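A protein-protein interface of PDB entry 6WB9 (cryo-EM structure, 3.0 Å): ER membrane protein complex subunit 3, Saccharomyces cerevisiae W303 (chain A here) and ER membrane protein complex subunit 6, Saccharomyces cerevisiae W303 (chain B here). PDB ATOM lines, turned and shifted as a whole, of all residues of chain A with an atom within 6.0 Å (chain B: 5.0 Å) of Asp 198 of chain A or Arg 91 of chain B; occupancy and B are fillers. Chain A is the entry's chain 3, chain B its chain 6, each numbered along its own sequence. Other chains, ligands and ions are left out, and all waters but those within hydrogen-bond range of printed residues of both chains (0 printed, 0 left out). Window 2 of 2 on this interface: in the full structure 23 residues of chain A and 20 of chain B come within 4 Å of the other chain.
Printed residues of chain B that touch a printed residue of chain A: Leu 25, Asp 29, Arg 91, Glu 92, Thr 94 and Gly 95. Hydrophobic or aromatic side chains of chain B within 4 Å of the printed part of chain A: Leu 25. Printed residues of chain A that touch a printed residue of chain B: Leu 185, Gly 186, Asn 188, Pro 189, Asn 192 and Asp 198. Hydrophobic or aromatic side chains of chain A within 4 Å of the printed part of chain B: Leu 185 and Pro 189. Among the printed residues, 11 pairs touch across the chains. Among the printed residues, Asp or Glu carboxylates within 4 Å of a Lys or Arg side-chain nitrogen of the other chain: Asp 198 of chain A with Arg 91 of chain B (2.4 Å).
Gly 186 of chain A touches Thr 94 of chain B (CA to O, 3.5 Å). CA of Gly 95 of chain B touches O of Gly 186 of chain A, 3.7 Å away. Pro 189 of chain A touches Asp 29 of chain B (CG to OD1, 3.3 Å). Glu 92 of chain B touches Pro 189 of chain A (OE1 to CG, 3.6 Å). CG of Pro 189 of chain A touches CA of Gly 95 of chain B, 3.997 Å away. Leu 25 of chain B touches Asn 192 of chain A (CD2 to OD1, 3.1 Å). CB of Asn 192 of chain A touches NH2 of Arg 91 of chain B, 3.4 Å away.
Asp 198 of chain A touches just one residue of chain B: Arg 91 (2.4 Å). Printed residues of chain A within 4 Å of Arg 91 of chain B: Asn 188 (2.9 Å), Asn 192 (3.4 Å) and Asp 198 (2.4 Å). Printed residues of chain A within 4 Å of Gly 95 of chain B: Gly 186 and Pro 189. Of the printed residues of chain B, Pro 189 of chain A touches Asp 29 (3.3 Å), Glu 92 (3.6 Å) and Gly 95 (3.997 Å). Of the printed residues of chain B, Gly 186 of chain A touches Thr 94 and Gly 95. Phe 90 of chain B touches none of the printed residues of chain A. The nearest printed residue of chain A that does not touch Arg 91 of chain B is Pro 189 of chain A (4.002 Å). The nearest printed residue of chain A that does not touch Leu 25 of chain B is Asp 198 of chain A (4.1 Å).
The backbone carbonyl oxygen (O) of Leu 185 of chain A lies within hydrogen-bond range of the side-chain hydroxyl (OG1) of Thr 94 of chain B. The backbone carbonyl oxygen (O) of Asn 188 of chain A is in hydrogen-bond range of the guanidinium group (NH2) of Arg 91 of chain B (2.9 Å). The side-chain carboxylate of Asp 29 of chain B is in hydrogen-bond range of the side-chain amide nitrogen of Asn 192 of chain A, at 2.8 Å. The side-chain carboxylate (OD2) of Asp 198 of chain A is in salt-bridge range of the guanidinium group (NH2) of Arg 91 of chain B.
The guanidinium group (NH2) of Arg 91 of chain B lies within salt-bridge range of the side-chain carboxylate (OD2) of Asp 29 of chain B, 3.3 Å away. The backbone NH of Asp 29 of chain B sits close to the side-chain carboxylate of Glu 92 of chain B (3.5 Å). The side-chain hydroxyl of Thr 94 of chain B is in hydrogen-bond range of the backbone carbonyl oxygen of Phe 90 of chain B, 2.9 Å away. NE of Arg 91 of chain B is in salt-bridge range of OE2 of Glu 92 of chain B. O of Arg 91 of chain B sits at hydrogen-bond distance from OG1 of Thr 94 of chain B, 2.8 Å away.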
ATOM      1  N   LEU A 185       5.816  -4.584  -8.771  1.00  0.00           N
ATOM      2  CA  LEU A 185       5.125  -3.376  -8.336  1.00  0.00           C
ATOM      3  C   LEU A 185       4.804  -3.416  -6.846  1.00  0.00           C
ATOM      4  O   LEU A 185       4.867  -2.389  -6.164  1.00  0.00           O
ATOM      5  CB  LEU A 185       3.844  -3.194  -9.147  1.00  0.00           C
ATOM      6  CG  LEU A 185       3.999  -3.098 -10.662  1.00  0.00           C
ATOM      7  CD1 LEU A 185       2.644  -3.190 -11.334  1.00  0.00           C
ATOM      8  CD2 LEU A 185       4.696  -1.802 -11.038  1.00  0.00           C
ATOM      9  N   GLY A 186       4.456  -4.586  -6.325  1.00  0.00           N
ATOM     10  CA  GLY A 186       3.868  -4.681  -5.008  1.00  0.00           C
ATOM     11  C   GLY A 186       4.748  -5.163  -3.878  1.00  0.00           C
ATOM     12  O   GLY A 186       4.236  -5.355  -2.772  1.00  0.00           O
ATOM     13  N   LEU A 187       6.047  -5.366  -4.098  1.00  0.00           N
ATOM     14  CA  LEU A 187       6.895  -5.854  -3.017  1.00  0.00           C
ATOM     15  C   LEU A 187       7.444  -4.745  -2.135  1.00  0.00           C
ATOM     16  O   LEU A 187       8.119  -5.052  -1.150  1.00  0.00           O
ATOM     17  CB  LEU A 187       8.068  -6.667  -3.563  1.00  0.00           C
ATOM     18  CG  LEU A 187       7.889  -8.180  -3.682  1.00  0.00           C
ATOM     19  CD1 LEU A 187       9.178  -8.829  -4.120  1.00  0.00           C
ATOM     20  CD2 LEU A 187       7.406  -8.774  -2.402  1.00  0.00           C
ATOM     21  N   ASN A 188       7.182  -3.482  -2.458  1.00  0.00           N
ATOM     22  CA  ASN A 188       7.643  -2.366  -1.637  1.00  0.00           C
ATOM     23  C   ASN A 188       6.992  -2.324  -0.248  1.00  0.00           C
ATOM     24  O   ASN A 188       7.691  -1.963   0.712  1.00  0.00           O
ATOM     25  CB  ASN A 188       7.441  -1.042  -2.379  1.00  0.00           C
ATOM     26  CG  ASN A 188       8.217  -0.978  -3.671  1.00  0.00           C
ATOM     27  OD1 ASN A 188       9.406  -1.286  -3.707  1.00  0.00           O
ATOM     28  ND2 ASN A 188       7.547  -0.584  -4.745  1.00  0.00           N
ATOM     29  N   PRO A 189       5.698  -2.669  -0.062  1.00  0.00           N
ATOM     30  CA  PRO A 189       5.243  -2.932   1.314  1.00  0.00           C
ATOM     31  C   PRO A 189       5.961  -4.081   1.997  1.00  0.00           C
ATOM     32  O   PRO A 189       6.272  -3.979   3.187  1.00  0.00           O
ATOM     33  CB  PRO A 189       3.753  -3.232   1.131  1.00  0.00           C
ATOM     34  CG  PRO A 189       3.371  -2.412   0.008  1.00  0.00           C
ATOM     35  CD  PRO A 189       4.521  -2.481  -0.941  1.00  0.00           C
ATOM     36  N   TYR A 191       9.003  -5.124   1.298  1.00  0.00           N
ATOM     37  CA  TYR A 191      10.363  -4.656   1.552  1.00  0.00           C
ATOM     38  C   TYR A 191      10.410  -3.732   2.760  1.00  0.00           C
ATOM     39  O   TYR A 191      11.369  -3.769   3.535  1.00  0.00           O
ATOM     40  CB  TYR A 191      10.919  -3.938   0.324  1.00  0.00           C
ATOM     41  CG  TYR A 191      11.259  -4.837  -0.839  1.00  0.00           C
ATOM     42  CD1 TYR A 191      11.695  -6.139  -0.637  1.00  0.00           C
ATOM     43  CD2 TYR A 191      11.147  -4.377  -2.143  1.00  0.00           C
ATOM     44  CE1 TYR A 191      12.007  -6.956  -1.702  1.00  0.00           C
ATOM     45  CE2 TYR A 191      11.454  -5.186  -3.213  1.00  0.00           C
ATOM     46  CZ  TYR A 191      11.883  -6.475  -2.987  1.00  0.00           C
ATOM     47  OH  TYR A 191      12.192  -7.282  -4.055  1.00  0.00           O
ATOM     48  N   ASN A 192       9.381  -2.905   2.942  1.00  0.00           N
ATOM     49  CA  ASN A 192       9.366  -2.004   4.088  1.00  0.00           C
ATOM     50  C   ASN A 192       9.085  -2.751   5.387  1.00  0.00           C
ATOM     51  O   ASN A 192       9.650  -2.414   6.432  1.00  0.00           O
ATOM     52  CB  ASN A 192       8.336  -0.903   3.864  1.00  0.00           C
ATOM     53  CG  ASN A 192       8.229   0.046   5.033  1.00  0.00           C
ATOM     54  OD1 ASN A 192       9.023   0.975   5.166  1.00  0.00           O
ATOM     55  ND2 ASN A 192       7.235  -0.172   5.884  1.00  0.00           N
ATOM     56  N   LEU A 196      13.940  -2.959   5.359  1.00  0.00           N
ATOM     57  CA  LEU A 196      14.933  -2.899   4.301  1.00  0.00           C
ATOM     58  C   LEU A 196      15.071  -1.534   3.642  1.00  0.00           C
ATOM     59  O   LEU A 196      15.977  -1.370   2.815  1.00  0.00           O
ATOM     60  CB  LEU A 196      14.615  -3.939   3.217  1.00  0.00           C
ATOM     61  CG  LEU A 196      15.787  -4.613   2.512  1.00  0.00           C
ATOM     62  CD1 LEU A 196      16.463  -5.595   3.448  1.00  0.00           C
ATOM     63  CD2 LEU A 196      15.307  -5.281   1.246  1.00  0.00           C
ATOM     64  N   ASN A 197      14.222  -0.558   3.992  1.00  0.00           N
ATOM     65  CA  ASN A 197      14.166   0.768   3.360  1.00  0.00           C
ATOM     66  C   ASN A 197      13.927   0.630   1.852  1.00  0.00           C
ATOM     67  O   ASN A 197      14.810   0.877   1.025  1.00  0.00           O
ATOM     68  CB  ASN A 197      15.410   1.612   3.676  1.00  0.00           C
ATOM     69  CG  ASN A 197      15.544   1.917   5.155  1.00  0.00           C
ATOM     70  OD1 ASN A 197      16.088   1.120   5.919  1.00  0.00           O
ATOM     71  ND2 ASN A 197      15.047   3.077   5.566  1.00  0.00           N
ATOM     72  N   ASP A 198      12.691   0.201   1.560  1.00  0.00           N
ATOM     73  CA  ASP A 198      12.188  -0.378   0.308  1.00  0.00           C
ATOM     74  C   ASP A 198      12.756   0.228  -0.970  1.00  0.00           C
ATOM     75  O   ASP A 198      12.823   1.451  -1.122  1.00  0.00           O
ATOM     76  CB  ASP A 198      10.668  -0.232   0.291  1.00  0.00           C
ATOM     77  CG  ASP A 198      10.225   1.163   0.672  1.00  0.00           C
ATOM     78  OD1 ASP A 198      10.461   1.568   1.829  1.00  0.00           O
ATOM     79  OD2 ASP A 198       9.665   1.866  -0.192  1.00  0.00           O
ATOM     80  N   GLN A 199      13.170  -0.650  -1.882  1.00  0.00           N
ATOM     81  CA  GLN A 199      13.716  -0.262  -3.179  1.00  0.00           C
ATOM     82  C   GLN A 199      12.677   0.437  -4.050  1.00  0.00           C
ATOM     83  O   GLN A 199      12.950   0.788  -5.197  1.00  0.00           O
ATOM     84  CB  GLN A 199      14.256  -1.494  -3.912  1.00  0.00           C
ATOM     85  CG  GLN A 199      15.394  -2.207  -3.195  1.00  0.00           C
ATOM     86  CD  GLN A 199      16.717  -1.467  -3.306  1.00  0.00           C
ATOM     87  OE1 GLN A 199      17.555  -1.537  -2.409  1.00  0.00           O
ATOM     88  NE2 GLN A 199      16.911  -0.762  -4.413  1.00  0.00           N
ATOM     89  N   LEU B  25       3.793   4.904   6.972  1.00  0.00           N
ATOM     90  CA  LEU B  25       4.105   3.918   5.949  1.00  0.00           C
ATOM     91  C   LEU B  25       4.006   2.505   6.493  1.00  0.00           C
ATOM     92  O   LEU B  25       3.578   1.603   5.773  1.00  0.00           O
ATOM     93  CB  LEU B  25       5.501   4.157   5.379  1.00  0.00           C
ATOM     94  CG  LEU B  25       6.017   3.164   4.340  1.00  0.00           C
ATOM     95  CD1 LEU B  25       5.142   3.204   3.104  1.00  0.00           C
ATOM     96  CD2 LEU B  25       7.464   3.438   3.985  1.00  0.00           C
ATOM     97  N   ASP B  29       1.426  -0.057   4.856  1.00  0.00           N
ATOM     98  CA  ASP B  29       1.963  -1.280   4.265  1.00  0.00           C
ATOM     99  C   ASP B  29       1.324  -2.521   4.869  1.00  0.00           C
ATOM    100  O   ASP B  29       0.897  -3.426   4.136  1.00  0.00           O
ATOM    101  CB  ASP B  29       3.481  -1.322   4.432  1.00  0.00           C
ATOM    102  CG  ASP B  29       4.192  -0.358   3.512  1.00  0.00           C
ATOM    103  OD1 ASP B  29       3.685  -0.106   2.405  1.00  0.00           O
ATOM    104  OD2 ASP B  29       5.254   0.160   3.896  1.00  0.00           O
ATOM    105  N   SER B  88       1.199   7.592  -1.058  1.00  0.00           N
ATOM    106  CA  SER B  88       1.431   6.157  -0.979  1.00  0.00           C
ATOM    107  C   SER B  88       0.257   5.393  -1.570  1.00  0.00           C
ATOM    108  O   SER B  88       0.119   4.197  -1.316  1.00  0.00           O
ATOM    109  CB  SER B  88       1.671   5.713   0.465  1.00  0.00           C
ATOM    110  OG  SER B  88       2.853   6.285   0.992  1.00  0.00           O
ATOM    111  N   PHE B  89      -0.587   6.063  -2.354  1.00  0.00           N
ATOM    112  CA  PHE B  89      -1.811   5.435  -2.834  1.00  0.00           C
ATOM    113  C   PHE B  89      -1.517   4.390  -3.900  1.00  0.00           C
ATOM    114  O   PHE B  89      -2.058   3.280  -3.855  1.00  0.00           O
ATOM    115  CB  PHE B  89      -2.772   6.489  -3.374  1.00  0.00           C
ATOM    116  CG  PHE B  89      -4.020   5.909  -3.959  1.00  0.00           C
ATOM    117  CD1 PHE B  89      -4.998   5.389  -3.133  1.00  0.00           C
ATOM    118  CD2 PHE B  89      -4.212   5.873  -5.332  1.00  0.00           C
ATOM    119  CE1 PHE B  89      -6.144   4.847  -3.659  1.00  0.00           C
ATOM    120  CE2 PHE B  89      -5.358   5.328  -5.867  1.00  0.00           C
ATOM    121  CZ  PHE B  89      -6.327   4.816  -5.029  1.00  0.00           C
ATOM    122  N   PHE B  90      -0.681   4.733  -4.880  1.00  0.00           N
ATOM    123  CA  PHE B  90      -0.313   3.759  -5.901  1.00  0.00           C
ATOM    124  C   PHE B  90       0.561   2.658  -5.325  1.00  0.00           C
ATOM    125  O   PHE B  90       0.439   1.498  -5.734  1.00  0.00           O
ATOM    126  CB  PHE B  90       0.390   4.454  -7.064  1.00  0.00           C
ATOM    127  CG  PHE B  90      -0.534   5.266  -7.925  1.00  0.00           C
ATOM    128  CD1 PHE B  90      -1.778   4.770  -8.283  1.00  0.00           C
ATOM    129  CD2 PHE B  90      -0.168   6.528  -8.363  1.00  0.00           C
ATOM    130  CE1 PHE B  90      -2.634   5.512  -9.071  1.00  0.00           C
ATOM    131  CE2 PHE B  90      -1.020   7.276  -9.152  1.00  0.00           C
ATOM    132  CZ  PHE B  90      -2.254   6.767  -9.506  1.00  0.00           C
ATOM    133  N   ARG B  91       1.397   2.994  -4.343  1.00  0.00           N
ATOM    134  CA  ARG B  91       2.232   2.003  -3.674  1.00  0.00           C
ATOM    135  C   ARG B  91       1.387   0.999  -2.900  1.00  0.00           C
ATOM    136  O   ARG B  91       1.588  -0.219  -3.008  1.00  0.00           O
ATOM    137  CB  ARG B  91       3.211   2.719  -2.750  1.00  0.00           C
ATOM    138  CG  ARG B  91       3.931   1.834  -1.771  1.00  0.00           C
ATOM    139  CD  ARG B  91       4.646   2.685  -0.748  1.00  0.00           C
ATOM    140  NE  ARG B  91       5.279   1.881   0.285  1.00  0.00           N
ATOM    141  CZ  ARG B  91       6.568   1.582   0.295  1.00  0.00           C
ATOM    142  NH1 ARG B  91       7.351   2.023  -0.675  1.00  0.00           N
ATOM    143  NH2 ARG B  91       7.072   0.846   1.270  1.00  0.00           N
ATOM    144  N   GLU B  92       0.402   1.489  -2.147  1.00  0.00           N
ATOM    145  CA  GLU B  92      -0.450   0.576  -1.402  1.00  0.00           C
ATOM    146  C   GLU B  92      -1.446  -0.142  -2.294  1.00  0.00           C
ATOM    147  O   GLU B  92      -1.854  -1.256  -1.966  1.00  0.00           O
ATOM    148  CB  GLU B  92      -1.199   1.299  -0.282  1.00  0.00           C
ATOM    149  CG  GLU B  92      -0.345   1.863   0.857  1.00  0.00           C
ATOM    150  CD  GLU B  92       0.960   1.129   1.099  1.00  0.00           C
ATOM    151  OE1 GLU B  92       0.943  -0.077   1.412  1.00  0.00           O
ATOM    152  OE2 GLU B  92       2.018   1.780   0.998  1.00  0.00           O
ATOM    153  N   ILE B  93      -1.821   0.435  -3.436  1.00  0.00           N
ATOM    154  CA  ILE B  93      -2.732  -0.297  -4.305  1.00  0.00           C
ATOM    155  C   ILE B  93      -1.979  -1.372  -5.086  1.00  0.00           C
ATOM    156  O   ILE B  93      -2.543  -2.430  -5.372  1.00  0.00           O
ATOM    157  CB  ILE B  93      -3.534   0.665  -5.208  1.00  0.00           C
ATOM    158  CG1 ILE B  93      -4.894   0.057  -5.541  1.00  0.00           C
ATOM    159  CG2 ILE B  93      -2.818   1.011  -6.502  1.00  0.00           C
ATOM    160  CD1 ILE B  93      -5.869   1.047  -6.108  1.00  0.00           C
ATOM    161  N   THR B  94      -0.680  -1.182  -5.355  1.00  0.00           N
ATOM    162  CA  THR B  94       0.096  -2.265  -5.944  1.00  0.00           C
ATOM    163  C   THR B  94       0.418  -3.347  -4.922  1.00  0.00           C
ATOM    164  O   THR B  94       0.423  -4.531  -5.271  1.00  0.00           O
ATOM    165  CB  THR B  94       1.383  -1.732  -6.571  1.00  0.00           C
ATOM    166  OG1 THR B  94       2.066  -0.887  -5.641  1.00  0.00           O
ATOM    167  CG2 THR B  94       1.074  -0.957  -7.837  1.00  0.00           C
ATOM    168  N   GLY B  95       0.660  -2.972  -3.662  1.00  0.00           N
ATOM    169  CA  GLY B  95       0.795  -3.976  -2.618  1.00  0.00           C
ATOM    170  C   GLY B  95      -0.487  -4.738  -2.350  1.00  0.00           C
ATOM    171  O   GLY B  95      -0.454  -5.945  -2.086  1.00  0.00           O
